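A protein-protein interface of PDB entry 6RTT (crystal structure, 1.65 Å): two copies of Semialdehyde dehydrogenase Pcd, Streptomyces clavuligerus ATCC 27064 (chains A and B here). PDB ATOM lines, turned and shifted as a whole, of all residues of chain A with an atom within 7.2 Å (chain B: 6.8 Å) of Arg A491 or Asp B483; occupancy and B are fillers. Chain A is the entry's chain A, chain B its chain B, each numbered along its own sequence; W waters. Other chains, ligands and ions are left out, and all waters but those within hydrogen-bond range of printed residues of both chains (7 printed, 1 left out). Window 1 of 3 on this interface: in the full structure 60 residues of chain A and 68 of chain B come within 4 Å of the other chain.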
ATOM      1  N   ARG A 136      26.888  19.316 -10.024  1.00  0.00           N
ATOM      2  CA  ARG A 136      27.280  18.256 -10.944  1.00  0.00           C
ATOM      3  C   ARG A 136      28.693  17.790 -10.647  1.00  0.00           C
ATOM      4  O   ARG A 136      29.524  18.546 -10.144  1.00  0.00           O
ATOM      5  CB  ARG A 136      27.201  18.729 -12.408  1.00  0.00           C
ATOM      6  CG  ARG A 136      25.771  19.034 -12.848  1.00  0.00           C
ATOM      7  CD  ARG A 136      25.651  19.657 -14.239  1.00  0.00           C
ATOM      8  NE  ARG A 136      24.246  19.600 -14.660  1.00  0.00           N
ATOM      9  CZ  ARG A 136      23.775  20.027 -15.827  1.00  0.00           C
ATOM     10  NH1 ARG A 136      24.589  20.579 -16.718  1.00  0.00           N
ATOM     11  NH2 ARG A 136      22.481  19.912 -16.098  1.00  0.00           N
ATOM     12  N   GLU A 149      30.894  20.888 -10.018  1.00  0.00           N
ATOM     13  CA  GLU A 149      30.197  22.160  -9.880  1.00  0.00           C
ATOM     14  C   GLU A 149      29.394  22.097  -8.591  1.00  0.00           C
ATOM     15  O   GLU A 149      28.636  21.152  -8.378  1.00  0.00           O
ATOM     16  CB  GLU A 149      29.289  22.407 -11.085  1.00  0.00           C
ATOM     17  CG  GLU A 149      28.344  23.585 -10.940  1.00  0.00           C
ATOM     18  CD  GLU A 149      27.307  23.600 -12.046  1.00  0.00           C
ATOM     19  OE1 GLU A 149      26.138  23.219 -11.789  1.00  0.00           O
ATOM     20  OE2 GLU A 149      27.687  23.969 -13.175  1.00  0.00           O
ATOM     21  N   THR A 150      29.588  23.073  -7.724  1.00  0.00           N
ATOM     22  CA  THR A 150      28.928  23.117  -6.433  1.00  0.00           C
ATOM     23  C   THR A 150      28.104  24.394  -6.336  1.00  0.00           C
ATOM     24  O   THR A 150      28.326  25.358  -7.072  1.00  0.00           O
ATOM     25  CB  THR A 150      29.948  23.027  -5.289  1.00  0.00           C
ATOM     26  OG1 THR A 150      30.957  24.034  -5.475  1.00  0.00           O
ATOM     27  CG2 THR A 150      30.624  21.650  -5.318  1.00  0.00           C
ATOM     28  N   TRP A 151      27.119  24.373  -5.446  1.00  0.00           N
ATOM     29  CA  TRP A 151      26.260  25.526  -5.217  1.00  0.00           C
ATOM     30  C   TRP A 151      26.364  25.948  -3.763  1.00  0.00           C
ATOM     31  O   TRP A 151      26.331  25.107  -2.850  1.00  0.00           O
ATOM     32  CB  TRP A 151      24.804  25.220  -5.609  1.00  0.00           C
ATOM     33  CG  TRP A 151      24.666  25.059  -7.097  1.00  0.00           C
ATOM     34  CD1 TRP A 151      24.882  23.915  -7.826  1.00  0.00           C
ATOM     35  CD2 TRP A 151      24.328  26.078  -8.040  1.00  0.00           C
ATOM     36  NE1 TRP A 151      24.684  24.169  -9.173  1.00  0.00           N
ATOM     37  CE2 TRP A 151      24.338  25.488  -9.326  1.00  0.00           C
ATOM     38  CE3 TRP A 151      24.004  27.437  -7.923  1.00  0.00           C
ATOM     39  CZ2 TRP A 151      24.041  26.210 -10.481  1.00  0.00           C
ATOM     40  CZ3 TRP A 151      23.703  28.152  -9.069  1.00  0.00           C
ATOM     41  CH2 TRP A 151      23.726  27.541 -10.333  1.00  0.00           C
ATOM     42  N   HIS A 152      26.482  27.255  -3.554  1.00  0.00           N
ATOM     43  CA  HIS A 152      26.728  27.806  -2.232  1.00  0.00           C
ATOM     44  C   HIS A 152      25.716  28.882  -1.881  1.00  0.00           C
ATOM     45  O   HIS A 152      25.227  29.596  -2.763  1.00  0.00           O
ATOM     46  CB  HIS A 152      28.140  28.402  -2.151  1.00  0.00           C
ATOM     47  CG  HIS A 152      29.213  27.405  -2.460  1.00  0.00           C
ATOM     48  ND1 HIS A 152      29.541  26.389  -1.595  1.00  0.00           N
ATOM     49  CD2 HIS A 152      30.003  27.247  -3.549  1.00  0.00           C
ATOM     50  CE1 HIS A 152      30.498  25.649  -2.129  1.00  0.00           C
ATOM     51  NE2 HIS A 152      30.796  26.149  -3.315  1.00  0.00           N
ATOM     52  N   LEU A 154      24.129  32.340  -0.987  1.00  0.00           N
ATOM     53  CA  LEU A 154      24.432  33.624  -1.609  1.00  0.00           C
ATOM     54  C   LEU A 154      24.575  34.753  -0.585  1.00  0.00           C
ATOM     55  O   LEU A 154      25.543  35.517  -0.636  1.00  0.00           O
ATOM     56  CB  LEU A 154      23.344  33.964  -2.629  1.00  0.00           C
ATOM     57  CG  LEU A 154      23.625  35.108  -3.598  1.00  0.00           C
ATOM     58  CD1 LEU A 154      24.687  34.685  -4.604  1.00  0.00           C
ATOM     59  CD2 LEU A 154      22.334  35.492  -4.328  1.00  0.00           C
ATOM     60  N   ARG A 261      21.910  40.750  -8.267  1.00  0.00           N
ATOM     61  CA  ARG A 261      21.031  39.891  -9.045  1.00  0.00           C
ATOM     62  C   ARG A 261      19.583  40.254  -8.733  1.00  0.00           C
ATOM     63  O   ARG A 261      19.267  40.622  -7.599  1.00  0.00           O
ATOM     64  CB  ARG A 261      21.309  38.415  -8.687  1.00  0.00           C
ATOM     65  CG  ARG A 261      20.599  37.375  -9.526  1.00  0.00           C
ATOM     66  CD  ARG A 261      20.875  35.968  -8.982  1.00  0.00           C
ATOM     67  NE  ARG A 261      22.286  35.591  -9.099  1.00  0.00           N
ATOM     68  CZ  ARG A 261      22.825  34.520  -8.521  1.00  0.00           C
ATOM     69  NH1 ARG A 261      22.079  33.729  -7.768  1.00  0.00           N
ATOM     70  NH2 ARG A 261      24.113  34.244  -8.682  1.00  0.00           N
ATOM     71  N   ASP A 483      14.030  24.234 -11.042  1.00  0.00           N
ATOM     72  CA  ASP A 483      15.286  24.650 -10.425  1.00  0.00           C
ATOM     73  C   ASP A 483      15.371  26.162 -10.255  1.00  0.00           C
ATOM     74  O   ASP A 483      16.458  26.746 -10.311  1.00  0.00           O
ATOM     75  CB  ASP A 483      16.489  24.106 -11.194  1.00  0.00           C
ATOM     76  CG  ASP A 483      16.502  24.498 -12.650  1.00  0.00           C
ATOM     77  OD1 ASP A 483      15.628  25.278 -13.098  1.00  0.00           O
ATOM     78  OD2 ASP A 483      17.427  24.022 -13.348  1.00  0.00           O
ATOM     79  N   ARG A 486      18.126  27.945  -8.042  1.00  0.00           N
ATOM     80  CA  ARG A 486      19.502  28.298  -8.394  1.00  0.00           C
ATOM     81  C   ARG A 486      19.733  29.798  -8.364  1.00  0.00           C
ATOM     82  O   ARG A 486      20.872  30.242  -8.150  1.00  0.00           O
ATOM     83  CB  ARG A 486      19.851  27.715  -9.763  1.00  0.00           C
ATOM     84  CG  ARG A 486      19.710  26.190  -9.788  1.00  0.00           C
ATOM     85  CD  ARG A 486      20.456  25.519 -10.937  1.00  0.00           C
ATOM     86  NE  ARG A 486      20.766  24.128 -10.586  1.00  0.00           N
ATOM     87  CZ  ARG A 486      20.271  23.053 -11.191  1.00  0.00           C
ATOM     88  NH1 ARG A 486      19.455  23.178 -12.229  1.00  0.00           N
ATOM     89  NH2 ARG A 486      20.610  21.840 -10.766  1.00  0.00           N
ATOM     90  N   MET A 489      21.434  30.964  -5.085  1.00  0.00           N
ATOM     91  CA  MET A 489      22.733  30.436  -4.700  1.00  0.00           C
ATOM     92  C   MET A 489      23.752  30.873  -5.740  1.00  0.00           C
ATOM     93  O   MET A 489      23.401  31.396  -6.803  1.00  0.00           O
ATOM     94  CB  MET A 489      22.686  28.905  -4.565  1.00  0.00           C
ATOM     95  CG  MET A 489      21.680  28.418  -3.489  1.00  0.00           C
ATOM     96  SD  MET A 489      21.746  26.644  -3.179  1.00  0.00           S
ATOM     97  CE  MET A 489      23.180  26.534  -2.115  1.00  0.00           C
ATOM     98  N   ARG A 490      25.031  30.676  -5.435  1.00  0.00           N
ATOM     99  CA  ARG A 490      26.079  30.958  -6.404  1.00  0.00           C
ATOM    100  C   ARG A 490      26.768  29.668  -6.823  1.00  0.00           C
ATOM    101  O   ARG A 490      27.037  28.791  -5.991  1.00  0.00           O
ATOM    102  CB  ARG A 490      27.105  31.958  -5.868  1.00  0.00           C
ATOM    103  CG  ARG A 490      27.724  31.591  -4.571  1.00  0.00           C
ATOM    104  CD  ARG A 490      28.912  32.524  -4.299  1.00  0.00           C
ATOM    105  NE  ARG A 490      29.366  32.359  -2.928  1.00  0.00           N
ATOM    106  CZ  ARG A 490      30.247  31.452  -2.535  1.00  0.00           C
ATOM    107  NH1 ARG A 490      30.792  30.625  -3.411  1.00  0.00           N
ATOM    108  NH2 ARG A 490      30.582  31.381  -1.254  1.00  0.00           N
ATOM    109  N   ARG A 491      27.018  29.566  -8.125  1.00  0.00           N
ATOM    110  CA  ARG A 491      27.670  28.406  -8.714  1.00  0.00           C
ATOM    111  C   ARG A 491      29.178  28.537  -8.547  1.00  0.00           C
ATOM    112  O   ARG A 491      29.737  29.627  -8.698  1.00  0.00           O
ATOM    113  CB  ARG A 491      27.305  28.326 -10.201  1.00  0.00           C
ATOM    114  CG  ARG A 491      27.787  27.094 -10.939  1.00  0.00           C
ATOM    115  CD  ARG A 491      27.763  27.303 -12.456  1.00  0.00           C
ATOM    116  NE  ARG A 491      26.485  27.812 -12.956  1.00  0.00           N
ATOM    117  CZ  ARG A 491      25.622  27.107 -13.683  1.00  0.00           C
ATOM    118  NH1 ARG A 491      25.889  25.842 -14.003  1.00  0.00           N
ATOM    119  NH2 ARG A 491      24.489  27.674 -14.092  1.00  0.00           N
ATOM    120  N   ALA A 492      29.837  27.425  -8.214  1.00  0.00           N
ATOM    121  CA  ALA A 492      31.293  27.363  -8.224  1.00  0.00           C
ATOM    122  C   ALA A 492      31.718  26.174  -9.070  1.00  0.00           C
ATOM    123  O   ALA A 492      31.113  25.101  -8.990  1.00  0.00           O
ATOM    124  CB  ALA A 492      31.873  27.249  -6.800  1.00  0.00           C
ATOM    125  N   THR A 493      32.733  26.382  -9.907  1.00  0.00           N
ATOM    126  CA  THR A 493      33.332  25.322 -10.706  1.00  0.00           C
ATOM    127  C   THR A 493      34.687  24.995 -10.097  1.00  0.00           C
ATOM    128  O   THR A 493      35.540  25.880  -9.996  1.00  0.00           O
ATOM    129  CB  THR A 493      33.487  25.765 -12.159  1.00  0.00           C
ATOM    130  OG1 THR A 493      32.202  26.132 -12.679  1.00  0.00           O
ATOM    131  CG2 THR A 493      34.075  24.643 -13.010  1.00  0.00           C
ATOM    132  N   PHE B 125      31.197  20.202 -28.236  1.00  0.00           N
ATOM    133  CA  PHE B 125      30.292  20.175 -27.091  1.00  0.00           C
ATOM    134  C   PHE B 125      28.895  20.632 -27.488  1.00  0.00           C
ATOM    135  O   PHE B 125      27.895  20.021 -27.090  1.00  0.00           O
ATOM    136  CB  PHE B 125      30.859  21.058 -25.976  1.00  0.00           C
ATOM    137  CG  PHE B 125      30.059  21.056 -24.699  1.00  0.00           C
ATOM    138  CD1 PHE B 125      30.189  20.027 -23.779  1.00  0.00           C
ATOM    139  CD2 PHE B 125      29.214  22.111 -24.400  1.00  0.00           C
ATOM    140  CE1 PHE B 125      29.466  20.037 -22.577  1.00  0.00           C
ATOM    141  CE2 PHE B 125      28.486  22.131 -23.210  1.00  0.00           C
ATOM    142  CZ  PHE B 125      28.618  21.096 -22.294  1.00  0.00           C
ATOM    143  N   LEU B 129      25.099  19.153 -27.235  1.00  0.00           N
ATOM    144  CA  LEU B 129      23.986  19.889 -26.640  1.00  0.00           C
ATOM    145  C   LEU B 129      22.780  19.939 -27.561  1.00  0.00           C
ATOM    146  O   LEU B 129      21.648  20.059 -27.082  1.00  0.00           O
ATOM    147  CB  LEU B 129      24.393  21.332 -26.310  1.00  0.00           C
ATOM    148  CG  LEU B 129      25.305  21.627 -25.122  1.00  0.00           C
ATOM    149  CD1 LEU B 129      25.514  23.138 -25.033  1.00  0.00           C
ATOM    150  CD2 LEU B 129      24.723  21.074 -23.815  1.00  0.00           C
ATOM    151  N   ASP B 449      35.153  32.683  -2.367  1.00  0.00           N
ATOM    152  CA  ASP B 449      33.851  33.134  -2.841  1.00  0.00           C
ATOM    153  C   ASP B 449      33.741  33.221  -4.365  1.00  0.00           C
ATOM    154  O   ASP B 449      32.736  33.737  -4.866  1.00  0.00           O
ATOM    155  CB  ASP B 449      33.508  34.508  -2.224  1.00  0.00           C
ATOM    156  CG  ASP B 449      34.430  35.644  -2.704  1.00  0.00           C
ATOM    157  OD1 ASP B 449      35.243  35.464  -3.654  1.00  0.00           O
ATOM    158  OD2 ASP B 449      34.330  36.763  -2.138  1.00  0.00           O
ATOM    159  N   CYS B 450      34.738  32.737  -5.108  1.00  0.00           N
ATOM    160  CA  CYS B 450      34.834  32.994  -6.536  1.00  0.00           C
ATOM    161  C   CYS B 450      34.010  32.001  -7.361  1.00  0.00           C
ATOM    162  O   CYS B 450      33.560  30.956  -6.880  1.00  0.00           O
ATOM    163  CB  CYS B 450      36.296  32.952  -6.967  1.00  0.00           C
ATOM    164  SG  CYS B 450      37.291  34.237  -6.169  1.00  0.00           S
ATOM    165  N   GLY B 451      33.795  32.355  -8.628  1.00  0.00           N
ATOM    166  CA  GLY B 451      33.087  31.456  -9.526  1.00  0.00           C
ATOM    167  C   GLY B 451      33.868  30.197  -9.852  1.00  0.00           C
ATOM    168  O   GLY B 451      33.276  29.155 -10.166  1.00  0.00           O
ATOM    169  N   ILE B 452      35.193  30.280  -9.809  1.00  0.00           N
ATOM    170  CA  ILE B 452      36.096  29.157 -10.045  1.00  0.00           C
ATOM    171  C   ILE B 452      36.965  29.031  -8.800  1.00  0.00           C
ATOM    172  O   ILE B 452      37.559  30.019  -8.361  1.00  0.00           O
ATOM    173  CB  ILE B 452      36.949  29.384 -11.311  1.00  0.00           C
ATOM    174  CG1 ILE B 452      36.065  29.363 -12.569  1.00  0.00           C
ATOM    175  CG2 ILE B 452      38.071  28.331 -11.413  1.00  0.00           C
ATOM    176  CD1 ILE B 452      36.723  29.975 -13.825  1.00  0.00           C
ATOM    177  N   GLY B 465      34.038  21.930 -20.412  1.00  0.00           N
ATOM    178  CA  GLY B 465      32.880  21.313 -19.773  1.00  0.00           C
ATOM    179  C   GLY B 465      32.374  22.030 -18.537  1.00  0.00           C
ATOM    180  O   GLY B 465      31.289  21.697 -18.048  1.00  0.00           O
ATOM    181  N   ALA B 467      31.132  25.549 -16.434  1.00  0.00           N
ATOM    182  CA  ALA B 467      30.607  26.899 -16.581  1.00  0.00           C
ATOM    183  C   ALA B 467      31.688  27.902 -16.199  1.00  0.00           C
ATOM    184  O   ALA B 467      32.300  27.788 -15.131  1.00  0.00           O
ATOM    185  CB  ALA B 467      29.368  27.081 -15.699  1.00  0.00           C
ATOM    186  N   PHE B 468      31.939  28.878 -17.070  1.00  0.00           N
ATOM    187  CA  PHE B 468      33.017  29.844 -16.867  1.00  0.00           C
ATOM    188  C   PHE B 468      32.454  31.217 -16.520  1.00  0.00           C
ATOM    189  O   PHE B 468      31.640  31.765 -17.268  1.00  0.00           O
ATOM    190  CB  PHE B 468      33.884  29.950 -18.122  1.00  0.00           C
ATOM    191  CG  PHE B 468      35.046  30.904 -17.989  1.00  0.00           C
ATOM    192  CD1 PHE B 468      34.904  32.247 -18.300  1.00  0.00           C
ATOM    193  CD2 PHE B 468      36.286  30.449 -17.580  1.00  0.00           C
ATOM    194  CE1 PHE B 468      35.973  33.124 -18.185  1.00  0.00           C
ATOM    195  CE2 PHE B 468      37.365  31.320 -17.469  1.00  0.00           C
ATOM    196  CZ  PHE B 468      37.204  32.657 -17.782  1.00  0.00           C
ATOM    197  N   GLY B 469      32.936  31.793 -15.427  1.00  0.00           N
ATOM    198  CA  GLY B 469      32.500  33.115 -15.025  1.00  0.00           C
ATOM    199  C   GLY B 469      32.675  33.291 -13.534  1.00  0.00           C
ATOM    200  O   GLY B 469      33.087  32.379 -12.823  1.00  0.00           O
ATOM    201  N   GLY B 470      32.338  34.495 -13.067  1.00  0.00           N
ATOM    202  CA  GLY B 470      32.572  34.783 -11.669  1.00  0.00           C
ATOM    203  C   GLY B 470      31.512  35.627 -10.999  1.00  0.00           C
ATOM    204  O   GLY B 470      30.462  35.911 -11.579  1.00  0.00           O
ATOM    205  N   GLU B 471      31.802  36.048  -9.775  1.00  0.00           N
ATOM    206  CA  GLU B 471      30.848  36.698  -8.898  1.00  0.00           C
ATOM    207  C   GLU B 471      31.263  38.143  -8.648  1.00  0.00           C
ATOM    208  O   GLU B 471      32.302  38.614  -9.121  1.00  0.00           O
ATOM    209  CB  GLU B 471      30.742  35.931  -7.578  1.00  0.00           C
ATOM    210  CG  GLU B 471      30.188  34.522  -7.761  1.00  0.00           C
ATOM    211  CD  GLU B 471      28.798  34.538  -8.369  1.00  0.00           C
ATOM    212  OE1 GLU B 471      27.902  35.190  -7.786  1.00  0.00           O
ATOM    213  OE2 GLU B 471      28.601  33.911  -9.436  1.00  0.00           O
ATOM    214  N   ARG B 478      27.743  33.250 -16.741  1.00  0.00           N
ATOM    215  CA  ARG B 478      28.451  32.006 -17.019  1.00  0.00           C
ATOM    216  C   ARG B 478      28.385  31.691 -18.507  1.00  0.00           C
ATOM    217  O   ARG B 478      27.348  31.888 -19.151  1.00  0.00           O
ATOM    218  CB  ARG B 478      27.882  30.809 -16.228  1.00  0.00           C
ATOM    219  CG  ARG B 478      28.086  30.897 -14.713  1.00  0.00           C
ATOM    220  CD  ARG B 478      29.562  30.857 -14.294  1.00  0.00           C
ATOM    221  NE  ARG B 478      29.705  30.824 -12.837  1.00  0.00           N
ATOM    222  CZ  ARG B 478      29.575  31.884 -12.038  1.00  0.00           C
ATOM    223  NH1 ARG B 478      29.279  33.078 -12.549  1.00  0.00           N
ATOM    224  NH2 ARG B 478      29.712  31.747 -10.723  1.00  0.00           N
ATOM    225  N   SER B 480      30.088  28.846 -21.773  1.00  0.00           N
ATOM    226  CA  SER B 480      30.687  27.567 -22.156  1.00  0.00           C
ATOM    227  C   SER B 480      29.904  26.370 -21.616  1.00  0.00           C
ATOM    228  O   SER B 480      28.853  26.022 -22.164  1.00  0.00           O
ATOM    229  CB  SER B 480      32.159  27.506 -21.718  1.00  0.00           C
ATOM    230  OG  SER B 480      32.812  26.382 -22.303  1.00  0.00           O
ATOM    231  N   GLY B 481      30.396  25.730 -20.553  1.00  0.00           N
ATOM    232  CA  GLY B 481      29.961  24.396 -20.174  1.00  0.00           C
ATOM    233  C   GLY B 481      28.818  24.312 -19.180  1.00  0.00           C
ATOM    234  O   GLY B 481      28.082  25.273 -18.939  1.00  0.00           O
ATOM    235  N   SER B 482      28.686  23.123 -18.585  1.00  0.00           N
ATOM    236  CA  SER B 482      27.542  22.751 -17.762  1.00  0.00           C
ATOM    237  C   SER B 482      26.274  23.176 -18.494  1.00  0.00           C
ATOM    238  O   SER B 482      26.172  22.963 -19.712  1.00  0.00           O
ATOM    239  CB  SER B 482      27.651  23.367 -16.360  1.00  0.00           C
ATOM    240  OG  SER B 482      26.699  22.809 -15.456  1.00  0.00           O
ATOM    241  N   ASP B 483      25.325  23.800 -17.798  1.00  0.00           N
ATOM    242  CA  ASP B 483      24.093  24.263 -18.431  1.00  0.00           C
ATOM    243  C   ASP B 483      24.092  25.778 -18.607  1.00  0.00           C
ATOM    244  O   ASP B 483      23.057  26.434 -18.510  1.00  0.00           O
ATOM    245  CB  ASP B 483      22.861  23.792 -17.659  1.00  0.00           C
ATOM    246  CG  ASP B 483      22.867  24.216 -16.212  1.00  0.00           C
ATOM    247  OD1 ASP B 483      23.765  24.981 -15.806  1.00  0.00           O
ATOM    248  OD2 ASP B 483      21.940  23.798 -15.483  1.00  0.00           O
ATOM    249  N   ALA B 484      25.267  26.342 -18.908  1.00  0.00           N
ATOM    250  CA  ALA B 484      25.336  27.752 -19.278  1.00  0.00           C
ATOM    251  C   ALA B 484      24.419  28.077 -20.445  1.00  0.00           C
ATOM    252  O   ALA B 484      23.959  29.216 -20.559  1.00  0.00           O
ATOM    253  CB  ALA B 484      26.776  28.144 -19.633  1.00  0.00           C
ATOM    254  N   TRP B 485      24.147  27.095 -21.321  1.00  0.00           N
ATOM    255  CA  TRP B 485      23.277  27.311 -22.475  1.00  0.00           C
ATOM    256  C   TRP B 485      21.905  27.855 -22.095  1.00  0.00           C
ATOM    257  O   TRP B 485      21.250  28.483 -22.935  1.00  0.00           O
ATOM    258  CB  TRP B 485      23.097  26.004 -23.259  1.00  0.00           C
ATOM    259  CG  TRP B 485      22.411  24.914 -22.483  1.00  0.00           C
ATOM    260  CD1 TRP B 485      23.018  23.904 -21.775  1.00  0.00           C
ATOM    261  CD2 TRP B 485      20.993  24.706 -22.334  1.00  0.00           C
ATOM    262  NE1 TRP B 485      22.069  23.102 -21.192  1.00  0.00           N
ATOM    263  CE2 TRP B 485      20.824  23.565 -21.522  1.00  0.00           C
ATOM    264  CE3 TRP B 485      19.857  25.373 -22.810  1.00  0.00           C
ATOM    265  CZ2 TRP B 485      19.561  23.080 -21.160  1.00  0.00           C
ATOM    266  CZ3 TRP B 485      18.601  24.889 -22.453  1.00  0.00           C
ATOM    267  CH2 TRP B 485      18.468  23.750 -21.630  1.00  0.00           C
ATOM    268  N   ARG B 486      21.452  27.642 -20.859  1.00  0.00           N
ATOM    269  CA  ARG B 486      20.111  28.090 -20.497  1.00  0.00           C
ATOM    270  C   ARG B 486      19.975  29.608 -20.603  1.00  0.00           C
ATOM    271  O   ARG B 486      18.871  30.118 -20.829  1.00  0.00           O
ATOM    272  CB  ARG B 486      19.755  27.613 -19.088  1.00  0.00           C
ATOM    273  CG  ARG B 486      19.571  26.108 -18.990  1.00  0.00           C
ATOM    274  CD  ARG B 486      19.086  25.692 -17.607  1.00  0.00           C
ATOM    275  NE  ARG B 486      19.205  24.245 -17.441  1.00  0.00           N
ATOM    276  CZ  ARG B 486      18.312  23.358 -17.870  1.00  0.00           C
ATOM    277  NH1 ARG B 486      17.226  23.766 -18.500  1.00  0.00           N
ATOM    278  NH2 ARG B 486      18.507  22.053 -17.680  1.00  0.00           N
ATOM    279  N   ALA B 487      21.073  30.347 -20.451  1.00  0.00           N
ATOM    280  CA  ALA B 487      20.973  31.800 -20.584  1.00  0.00           C
ATOM    281  C   ALA B 487      20.678  32.235 -22.009  1.00  0.00           C
ATOM    282  O   ALA B 487      20.348  33.406 -22.234  1.00  0.00           O
ATOM    283  CB  ALA B 487      22.263  32.468 -20.096  1.00  0.00           C
HETATM  284  O   HOH W   1      30.433  24.285 -13.947  1.00  0.00           O
HETATM  285  O   HOH W   2      30.818  30.842  -6.475  1.00  0.00           O
HETATM  286  O   HOH W   3      26.300  34.055 -10.512  1.00  0.00           O
HETATM  287  O   HOH W   4      22.343  28.066 -16.330  1.00  0.00           O
HETATM  288  O   HOH W   5      24.054  22.833 -13.440  1.00  0.00           O
HETATM  289  O   HOH W   6      30.998  28.609 -11.681  1.00  0.00           O
HETATM  290  O   HOH W   7      33.717  29.227  -4.624  1.00  0.00           O
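Positions printed for both chains: 483 and 486. Of the 14 pairs that touch across the chains among the printed residues, none has its exchanged pair printed and touching as well.
Of the printed residues of chain B, Arg A136 touches Ser B482 and Asp B483. Printed residues of chain B within 4 Å of Arg A491: Gly B451 (3.9 Å), Ala B467 (3.6 Å), Arg B478 (2.9 Å), Ser B482 (3.5 Å) and Asp B483 (2.9 Å). Of the printed residues of chain A, Ser B482 touches Arg A136, Glu A149 and Arg A491. The nearest residue of chain B that does not touch Arg A491 is Cys B450 (4.4 Å). The nearest printed residue of chain B that does not touch Arg A136 is Arg B486 (4.8 Å).
The backbone NH (N) of Ser B482 sits at hydrogen-bond distance from the backbone carbonyl oxygen (O) of Gly B465 (3.0 Å). The side-chain carboxylate (OE2) of Glu A149 is in salt-bridge range of the guanidinium group (NH1) of Arg A491, 2.7 Å away. N of Arg A490 sits at hydrogen-bond distance from O of His A152 (2.9 Å). OE2 of Glu B471 is in salt-bridge range of NH2 of Arg B478 (2.8 Å). The backbone NH of Glu A149 sits at hydrogen-bond distance from the backbone carbonyl oxygen of Arg A136, at 2.7 Å. NE of Arg B486 lies within salt-bridge range of OD2 of Asp B483, at 3.4 Å.
Arg A490 touches Asp B449. Glu B471 touches Arg A490. Gly B451 touches Arg A491. CB of Ala B467 touches CD of Arg A491, 3.6 Å away. Ala A492 touches Gly B451 (CA to O, 3.3 Å). Thr A493 touches Ile B452 (O to CA, 3.3 Å).
The side-chain hydroxyl of Ser B482 sits at hydrogen-bond distance from the guanidinium group of Arg A491 (3.5 Å). The side-chain hydroxyl (OG1) of Thr A493 is in hydrogen-bond range of the backbone carbonyl oxygen (O) of Ala B467, at 3.0 Å. The guanidinium group (NH2) of Arg B478 lies within hydrogen-bond range of the backbone carbonyl oxygen (O) of Arg A491. OE2 of Glu A149 is in hydrogen-bond range of OG of Ser B482 (2.7 Å). OD2 of Asp B483 is in salt-bridge range of NH2 of Arg A136 (3.97 Å). The side-chain carboxylate (OD1) of Asp B483 is in salt-bridge range of the guanidinium group (NH1) of Arg A491 (2.9 Å). The backbone NH of Thr A493 is in hydrogen-bond range of the backbone carbonyl oxygen of Gly B451 (2.8 Å). NH1 of Arg A136 is in hydrogen-bond range of OG of Ser B482, 3.3 Å away.
Printed residues of chain A that touch a printed residue of chain B: Arg A136, Glu A149, Arg A490, Arg A491, Ala A492 and Thr A493. Printed residues of chain B that touch a printed residue of chain A: Asp B449, Gly B451, Ile B452, Ala B467, Glu B471, Arg B478, Ser B482 and Asp B483. Hydrophobic or aromatic side chains of chain B that line the printed part of chain A: Ile B452 and Ala B467. Along chain B the printed residues that touch a printed residue of chain A span positions 449 to 483. Among the printed residues, 14 pairs touch across the chains. Among the printed residues, Asp or Glu carboxylates within 4 Å of a Lys or Arg side-chain nitrogen of the other chain: Arg A136 with Asp B483 (3.97 Å) and Arg A491 with Asp B483 (2.9 Å).
Water W3 bridges the side-chain carboxylate (OE2) of Glu B471 and the guanidinium group (NH2) of Arg A261. Water W5 lies within hydrogen-bond range of OE1 of Glu A149 (2.7 Å), OD2 of Asp B483 (3.1 Å), OG of Ser B482 (3.3 Å) and NE of Arg A136 (3.5 Å). Water W6 lies within hydrogen-bond range of the backbone carbonyl oxygen (O) of Gly B451, the guanidinium group (NE) of Arg B478, the side-chain hydroxyl (OG1) of Thr A493 and the backbone carbonyl oxygen (O) of Arg A491. Water W4 bridges O of Asp B483 (2.8 Å) and NH2 of Arg A491 (3.1 Å). Water W7 lies within hydrogen-bond range of O of Cys B450 (2.8 Å) and NH1 of Arg A490 (3.5 Å). Water W1 lies within hydrogen-bond range of the side-chain hydroxyl (OG1) of Thr A493, the side-chain carboxylate (OE2) of Glu A149 and the backbone NH (N) of Ala B467.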
